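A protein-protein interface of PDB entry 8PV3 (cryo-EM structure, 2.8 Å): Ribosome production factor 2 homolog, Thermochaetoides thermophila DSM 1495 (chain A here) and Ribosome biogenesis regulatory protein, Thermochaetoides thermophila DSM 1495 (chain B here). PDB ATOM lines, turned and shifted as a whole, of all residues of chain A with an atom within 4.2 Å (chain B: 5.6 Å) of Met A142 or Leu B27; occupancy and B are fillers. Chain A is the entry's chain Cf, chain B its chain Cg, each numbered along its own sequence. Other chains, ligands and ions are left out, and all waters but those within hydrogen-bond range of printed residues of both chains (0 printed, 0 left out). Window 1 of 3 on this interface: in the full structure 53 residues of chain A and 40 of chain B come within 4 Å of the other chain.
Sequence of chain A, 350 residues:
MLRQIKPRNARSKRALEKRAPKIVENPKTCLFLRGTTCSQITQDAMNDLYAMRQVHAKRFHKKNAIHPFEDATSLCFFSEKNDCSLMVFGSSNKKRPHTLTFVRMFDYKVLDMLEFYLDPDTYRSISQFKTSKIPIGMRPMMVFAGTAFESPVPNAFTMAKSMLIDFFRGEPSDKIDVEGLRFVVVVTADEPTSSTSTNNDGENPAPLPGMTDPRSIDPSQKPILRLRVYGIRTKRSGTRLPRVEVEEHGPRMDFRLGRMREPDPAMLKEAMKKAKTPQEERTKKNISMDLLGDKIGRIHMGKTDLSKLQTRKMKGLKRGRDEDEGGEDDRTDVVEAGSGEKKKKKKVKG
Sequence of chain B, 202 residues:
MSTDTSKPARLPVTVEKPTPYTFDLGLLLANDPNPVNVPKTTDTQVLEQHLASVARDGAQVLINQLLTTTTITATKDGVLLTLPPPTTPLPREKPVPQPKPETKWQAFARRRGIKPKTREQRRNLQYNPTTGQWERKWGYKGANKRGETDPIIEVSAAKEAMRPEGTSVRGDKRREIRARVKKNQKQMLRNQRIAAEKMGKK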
ATOM      1  N   ARG A 139      25.550  13.844 -12.831  1.00  0.00           N
ATOM      2  CA  ARG A 139      24.615  13.128 -13.687  1.00  0.00           C
ATOM      3  C   ARG A 139      23.246  13.022 -13.014  1.00  0.00           C
ATOM      4  O   ARG A 139      23.162  12.882 -11.792  1.00  0.00           O
ATOM      5  CB  ARG A 139      25.145  11.734 -14.016  1.00  0.00           C
ATOM      6  CG  ARG A 139      25.543  10.922 -12.799  1.00  0.00           C
ATOM      7  CD  ARG A 139      26.011   9.532 -13.167  1.00  0.00           C
ATOM      8  NE  ARG A 139      24.909   8.694 -13.617  1.00  0.00           N
ATOM      9  CZ  ARG A 139      25.054   7.479 -14.128  1.00  0.00           C
ATOM     10  NH1 ARG A 139      26.246   6.919 -14.249  1.00  0.00           N
ATOM     11  NH2 ARG A 139      23.976   6.808 -14.521  1.00  0.00           N
ATOM     12  N   PRO A 140      22.165  13.105 -13.783  1.00  0.00           N
ATOM     13  CA  PRO A 140      20.829  12.891 -13.228  1.00  0.00           C
ATOM     14  C   PRO A 140      20.369  11.451 -13.402  1.00  0.00           C
ATOM     15  O   PRO A 140      20.974  10.654 -14.121  1.00  0.00           O
ATOM     16  CB  PRO A 140      19.966  13.841 -14.066  1.00  0.00           C
ATOM     17  CG  PRO A 140      20.621  13.806 -15.405  1.00  0.00           C
ATOM     18  CD  PRO A 140      22.104  13.594 -15.172  1.00  0.00           C
ATOM     19  N   MET A 141      19.273  11.126 -12.724  1.00  0.00           N
ATOM     20  CA  MET A 141      18.618   9.854 -12.983  1.00  0.00           C
ATOM     21  C   MET A 141      17.681   9.994 -14.177  1.00  0.00           C
ATOM     22  O   MET A 141      17.348  11.099 -14.604  1.00  0.00           O
ATOM     23  CB  MET A 141      17.843   9.362 -11.763  1.00  0.00           C
ATOM     24  CG  MET A 141      17.134  10.440 -10.985  1.00  0.00           C
ATOM     25  SD  MET A 141      16.555   9.838  -9.396  1.00  0.00           S
ATOM     26  CE  MET A 141      18.115   9.425  -8.636  1.00  0.00           C
ATOM     27  N   MET A 142      17.262   8.856 -14.720  1.00  0.00           N
ATOM     28  CA  MET A 142      16.444   8.832 -15.922  1.00  0.00           C
ATOM     29  C   MET A 142      15.180   8.019 -15.689  1.00  0.00           C
ATOM     30  O   MET A 142      15.221   6.956 -15.064  1.00  0.00           O
ATOM     31  CB  MET A 142      17.220   8.251 -17.102  1.00  0.00           C
ATOM     32  CG  MET A 142      18.376   9.118 -17.558  1.00  0.00           C
ATOM     33  SD  MET A 142      19.225   8.434 -18.987  1.00  0.00           S
ATOM     34  CE  MET A 142      20.124   7.095 -18.220  1.00  0.00           C
ATOM     35  N   VAL A 143      14.059   8.529 -16.195  1.00  0.00           N
ATOM     36  CA  VAL A 143      12.774   7.842 -16.149  1.00  0.00           C
ATOM     37  C   VAL A 143      12.156   7.918 -17.538  1.00  0.00           C
ATOM     38  O   VAL A 143      11.946   9.016 -18.067  1.00  0.00           O
ATOM     39  CB  VAL A 143      11.827   8.450 -15.100  1.00  0.00           C
ATOM     40  CG1 VAL A 143      10.425   7.887 -15.260  1.00  0.00           C
ATOM     41  CG2 VAL A 143      12.342   8.185 -13.693  1.00  0.00           C
ATOM     42  N   ILE A 165      19.374   7.864 -23.613  1.00  0.00           N
ATOM     43  CA  ILE A 165      20.111   7.193 -22.547  1.00  0.00           C
ATOM     44  C   ILE A 165      21.610   7.399 -22.726  1.00  0.00           C
ATOM     45  O   ILE A 165      22.329   7.687 -21.762  1.00  0.00           O
ATOM     46  CB  ILE A 165      19.735   5.700 -22.500  1.00  0.00           C
ATOM     47  CG1 ILE A 165      18.352   5.516 -21.879  1.00  0.00           C
ATOM     48  CG2 ILE A 165      20.756   4.891 -21.717  1.00  0.00           C
ATOM     49  CD1 ILE A 165      17.801   4.128 -22.051  1.00  0.00           C
ATOM     50  N   PHE A 168      22.398  11.136 -21.745  1.00  0.00           N
ATOM     51  CA  PHE A 168      22.337  11.429 -20.318  1.00  0.00           C
ATOM     52  C   PHE A 168      23.024  10.370 -19.465  1.00  0.00           C
ATOM     53  O   PHE A 168      22.815  10.339 -18.248  1.00  0.00           O
ATOM     54  CB  PHE A 168      20.884  11.588 -19.871  1.00  0.00           C
ATOM     55  CG  PHE A 168      20.215  12.820 -20.407  1.00  0.00           C
ATOM     56  CD1 PHE A 168      20.519  14.067 -19.892  1.00  0.00           C
ATOM     57  CD2 PHE A 168      19.279  12.729 -21.421  1.00  0.00           C
ATOM     58  CE1 PHE A 168      19.906  15.202 -20.383  1.00  0.00           C
ATOM     59  CE2 PHE A 168      18.663  13.860 -21.916  1.00  0.00           C
ATOM     60  CZ  PHE A 168      18.976  15.096 -21.396  1.00  0.00           C
ATOM     61  N   ARG A 169      23.822   9.494 -20.079  1.00  0.00           N
ATOM     62  CA  ARG A 169      24.468   8.412 -19.342  1.00  0.00           C
ATOM     63  C   ARG A 169      25.498   8.940 -18.351  1.00  0.00           C
ATOM     64  O   ARG A 169      25.600   8.439 -17.226  1.00  0.00           O
ATOM     65  CB  ARG A 169      25.111   7.438 -20.327  1.00  0.00           C
ATOM     66  CG  ARG A 169      25.754   6.222 -19.698  1.00  0.00           C
ATOM     67  CD  ARG A 169      26.311   5.301 -20.766  1.00  0.00           C
ATOM     68  NE  ARG A 169      26.904   4.101 -20.193  1.00  0.00           N
ATOM     69  CZ  ARG A 169      28.174   3.998 -19.827  1.00  0.00           C
ATOM     70  NH1 ARG A 169      29.016   5.010 -19.962  1.00  0.00           N
ATOM     71  NH2 ARG A 169      28.611   2.852 -19.314  1.00  0.00           N
ATOM     72  N   VAL A 185      15.461  13.183 -15.145  1.00  0.00           N
ATOM     73  CA  VAL A 185      15.100  13.505 -16.519  1.00  0.00           C
ATOM     74  C   VAL A 185      14.049  12.507 -16.976  1.00  0.00           C
ATOM     75  O   VAL A 185      14.303  11.298 -17.004  1.00  0.00           O
ATOM     76  CB  VAL A 185      16.329  13.467 -17.438  1.00  0.00           C
ATOM     77  CG1 VAL A 185      15.920  13.705 -18.867  1.00  0.00           C
ATOM     78  CG2 VAL A 185      17.347  14.499 -16.999  1.00  0.00           C
ATOM     79  N   ASP B  24      17.301  -0.361 -14.171  1.00  0.00           N
ATOM     80  CA  ASP B  24      18.718  -0.562 -14.465  1.00  0.00           C
ATOM     81  C   ASP B  24      19.452   0.409 -13.542  1.00  0.00           C
ATOM     82  O   ASP B  24      19.671   1.576 -13.873  1.00  0.00           O
ATOM     83  CB  ASP B  24      19.047  -0.317 -15.933  1.00  0.00           C
ATOM     84  CG  ASP B  24      20.482  -0.662 -16.270  1.00  0.00           C
ATOM     85  OD1 ASP B  24      21.106  -1.423 -15.503  1.00  0.00           O
ATOM     86  OD2 ASP B  24      20.990  -0.165 -17.294  1.00  0.00           O
ATOM     87  N   LEU B  25      19.812  -0.075 -12.353  1.00  0.00           N
ATOM     88  CA  LEU B  25      20.346   0.812 -11.329  1.00  0.00           C
ATOM     89  C   LEU B  25      21.789   1.215 -11.602  1.00  0.00           C
ATOM     90  O   LEU B  25      22.294   2.137 -10.954  1.00  0.00           O
ATOM     91  CB  LEU B  25      20.222   0.150  -9.957  1.00  0.00           C
ATOM     92  CG  LEU B  25      18.793  -0.240  -9.566  1.00  0.00           C
ATOM     93  CD1 LEU B  25      18.742  -0.737  -8.134  1.00  0.00           C
ATOM     94  CD2 LEU B  25      17.833   0.925  -9.758  1.00  0.00           C
ATOM     95  N   GLY B  26      22.465   0.544 -12.536  1.00  0.00           N
ATOM     96  CA  GLY B  26      23.779   0.998 -12.951  1.00  0.00           C
ATOM     97  C   GLY B  26      23.739   2.318 -13.694  1.00  0.00           C
ATOM     98  O   GLY B  26      24.621   3.161 -13.520  1.00  0.00           O
ATOM     99  N   LEU B  27      22.722   2.515 -14.531  1.00  0.00           N
ATOM    100  CA  LEU B  27      22.525   3.760 -15.258  1.00  0.00           C
ATOM    101  C   LEU B  27      21.517   4.674 -14.579  1.00  0.00           C
ATOM    102  O   LEU B  27      21.197   5.734 -15.129  1.00  0.00           O
ATOM    103  CB  LEU B  27      22.076   3.472 -16.690  1.00  0.00           C
ATOM    104  CG  LEU B  27      22.988   2.581 -17.527  1.00  0.00           C
ATOM    105  CD1 LEU B  27      22.427   2.425 -18.928  1.00  0.00           C
ATOM    106  CD2 LEU B  27      24.394   3.151 -17.567  1.00  0.00           C
ATOM    107  N   LEU B  28      21.024   4.287 -13.395  1.00  0.00           N
ATOM    108  CA  LEU B  28      19.957   4.991 -12.675  1.00  0.00           C
ATOM    109  C   LEU B  28      18.726   5.182 -13.555  1.00  0.00           C
ATOM    110  O   LEU B  28      18.104   6.244 -13.573  1.00  0.00           O
ATOM    111  CB  LEU B  28      20.446   6.331 -12.121  1.00  0.00           C
ATOM    112  CG  LEU B  28      21.744   6.303 -11.315  1.00  0.00           C
ATOM    113  CD1 LEU B  28      22.233   7.716 -11.076  1.00  0.00           C
ATOM    114  CD2 LEU B  28      21.544   5.571 -10.001  1.00  0.00           C
ATOM    115  N   LEU B  29      18.374   4.136 -14.296  1.00  0.00           N
ATOM    116  CA  LEU B  29      17.308   4.183 -15.283  1.00  0.00           C
ATOM    117  C   LEU B  29      16.091   3.438 -14.756  1.00  0.00           C
ATOM    118  O   LEU B  29      16.211   2.308 -14.272  1.00  0.00           O
ATOM    119  CB  LEU B  29      17.774   3.566 -16.603  1.00  0.00           C
ATOM    120  CG  LEU B  29      16.703   3.282 -17.652  1.00  0.00           C
ATOM    121  CD1 LEU B  29      16.124   4.578 -18.181  1.00  0.00           C
ATOM    122  CD2 LEU B  29      17.270   2.438 -18.777  1.00  0.00           C
ATOM    123  N   ALA B  30      14.928   4.072 -14.844  1.00  0.00           N
ATOM    124  CA  ALA B  30      13.661   3.441 -14.506  1.00  0.00           C
ATOM    125  C   ALA B  30      12.771   3.458 -15.738  1.00  0.00           C
ATOM    126  O   ALA B  30      12.552   4.518 -16.332  1.00  0.00           O
ATOM    127  CB  ALA B  30      12.975   4.156 -13.341  1.00  0.00           C
ATOM    128  N   LEU B  62      12.102   4.926  -8.139  1.00  0.00           N
ATOM    129  CA  LEU B  62      13.548   4.801  -8.316  1.00  0.00           C
ATOM    130  C   LEU B  62      14.288   5.002  -6.997  1.00  0.00           C
ATOM    131  O   LEU B  62      15.228   4.261  -6.682  1.00  0.00           O
ATOM    132  CB  LEU B  62      14.034   5.797  -9.368  1.00  0.00           C
ATOM    133  CG  LEU B  62      15.468   5.616  -9.864  1.00  0.00           C
ATOM    134  CD1 LEU B  62      15.758   4.159 -10.179  1.00  0.00           C
ATOM    135  CD2 LEU B  62      15.690   6.472 -11.087  1.00  0.00           C
ATOM    136  N   PRO B  86      25.683  -1.998 -15.333  1.00  0.00           N
ATOM    137  CA  PRO B  86      24.534  -1.687 -16.193  1.00  0.00           C
ATOM    138  C   PRO B  86      24.108  -2.875 -17.043  1.00  0.00           C
ATOM    139  O   PRO B  86      24.934  -3.670 -17.495  1.00  0.00           O
ATOM    140  CB  PRO B  86      25.048  -0.535 -17.064  1.00  0.00           C
ATOM    141  CG  PRO B  86      26.192   0.043 -16.299  1.00  0.00           C
ATOM    142  CD  PRO B  86      26.829  -1.118 -15.610  1.00  0.00           C
ATOM    143  N   THR B  87      22.798  -2.988 -17.255  1.00  0.00           N
ATOM    144  CA  THR B  87      22.224  -4.070 -18.044  1.00  0.00           C
ATOM    145  C   THR B  87      21.554  -3.601 -19.324  1.00  0.00           C
ATOM    146  O   THR B  87      21.270  -4.429 -20.192  1.00  0.00           O
ATOM    147  CB  THR B  87      21.197  -4.853 -17.216  1.00  0.00           C
ATOM    148  OG1 THR B  87      20.129  -3.982 -16.825  1.00  0.00           O
ATOM    149  CG2 THR B  87      21.848  -5.439 -15.974  1.00  0.00           C
ATOM    150  N   THR B  88      21.289  -2.307 -19.460  1.00  0.00           N
ATOM    151  CA  THR B  88      20.722  -1.782 -20.691  1.00  0.00           C
ATOM    152  C   THR B  88      21.772  -1.841 -21.794  1.00  0.00           C
ATOM    153  O   THR B  88      22.868  -1.284 -21.626  1.00  0.00           O
ATOM    154  CB  THR B  88      20.239  -0.346 -20.503  1.00  0.00           C
ATOM    155  OG1 THR B  88      19.201  -0.317 -19.517  1.00  0.00           O
ATOM    156  CG2 THR B  88      19.700   0.208 -21.812  1.00  0.00           C
ATOM    157  N   LEU B  90      23.931  -0.885 -24.840  1.00  0.00           N
ATOM    158  CA  LEU B  90      24.268   0.351 -25.529  1.00  0.00           C
ATOM    159  C   LEU B  90      25.430   0.094 -26.474  1.00  0.00           C
ATOM    160  O   LEU B  90      26.315  -0.714 -26.167  1.00  0.00           O
ATOM    161  CB  LEU B  90      24.643   1.466 -24.539  1.00  0.00           C
ATOM    162  CG  LEU B  90      23.491   2.082 -23.745  1.00  0.00           C
ATOM    163  CD1 LEU B  90      24.020   2.892 -22.578  1.00  0.00           C
ATOM    164  CD2 LEU B  90      22.623   2.940 -24.644  1.00  0.00           C
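The guanidinium group (NH2) of Arg A139 is in hydrogen-bond range of the backbone carbonyl oxygen (O) of Leu B27.
N of Met A142 lies within hydrogen-bond range of O of Leu B28, at 3.0 Å.
N of Ala B30 lies within hydrogen-bond range of O of Met A142.
The guanidinium group (NH1) of Arg A139 lies close to the backbone carbonyl oxygen (O) of Arg A169 (3.4 Å).
The backbone NH (N) of Val A185 lies within hydrogen-bond range of the backbone carbonyl oxygen (O) of Met A141 (2.9 Å).
The backbone carbonyl oxygen (O) of Val A185 lies within hydrogen-bond range of the backbone NH (N) of Val A143.
N of Asp B24 sits at hydrogen-bond distance from O of Leu B29 (2.9 Å).
O of Gly B26 touches NH2 of Arg A139, at 3.8 Å.
Leu B28 touches Met A141.
Leu B62 touches Met A141 (CD2 to CB, 3.7 Å).
Leu B27 touches Met A142 (O to CE, 3.5 Å).
Met A142 touches Leu B29 (O to CA, 3.5 Å).
CA of Val A143 touches O of Ala B30 (3.3 Å).
Ile A165 touches Leu B29.
Ile A165 touches Leu B90 (CG2 to CD1, 3.9 Å).
Leu B27 touches Arg A169.
Leu B90 touches Arg A169 (CD1 to CD, 3.8 Å).
Of chain B, only Leu B27 (3.5 Å), Leu B28 (3.0 Å), Leu B29 (3.5 Å) and Ala B30 (2.9 Å) come within 4 Å of Met A142.
Leu B27 touches just these residues of chain A: Arg A139, Met A142 and Arg A169.
Printed residues of chain B within 4 Å of Met A141: Leu B28 and Leu B62.
Of the printed residues of chain A, Leu B90 touches Ile A165 and Arg A169.
Printed residues of chain B within 4 Å of Ile A165: Leu B29 (3.7 Å) and Leu B90 (3.9 Å).
The nearest residue of chain B that does not touch Met A142 is Leu B62 (4.03 Å).
Of the 9 printed residues of chain A, 6 touch a printed residue of chain B.
Hydrophobic or aromatic side chains of chain A within 4 Å of the printed part of chain B: Met A141, Met A142 and Ile A165.
Of the 12 printed residues of chain B, 7 touch a printed residue of chain A.
Printed residues of chain B that touch a printed residue of chain A: Gly B26, Leu B27, Leu B28, Leu B29, Ala B30, Leu B62 and Leu B90.
Hydrophobic or aromatic side chains of chain B that line the printed part of chain A: Leu B27, Leu B28, Leu B29, Ala B30, Leu B62 and Leu B90.
Among the printed residues, 14 pairs touch across the chains.
Among the printed residues, no Asp or Glu carboxylate lies within 4 Å of a Lys or Arg side-chain nitrogen of the other chain.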
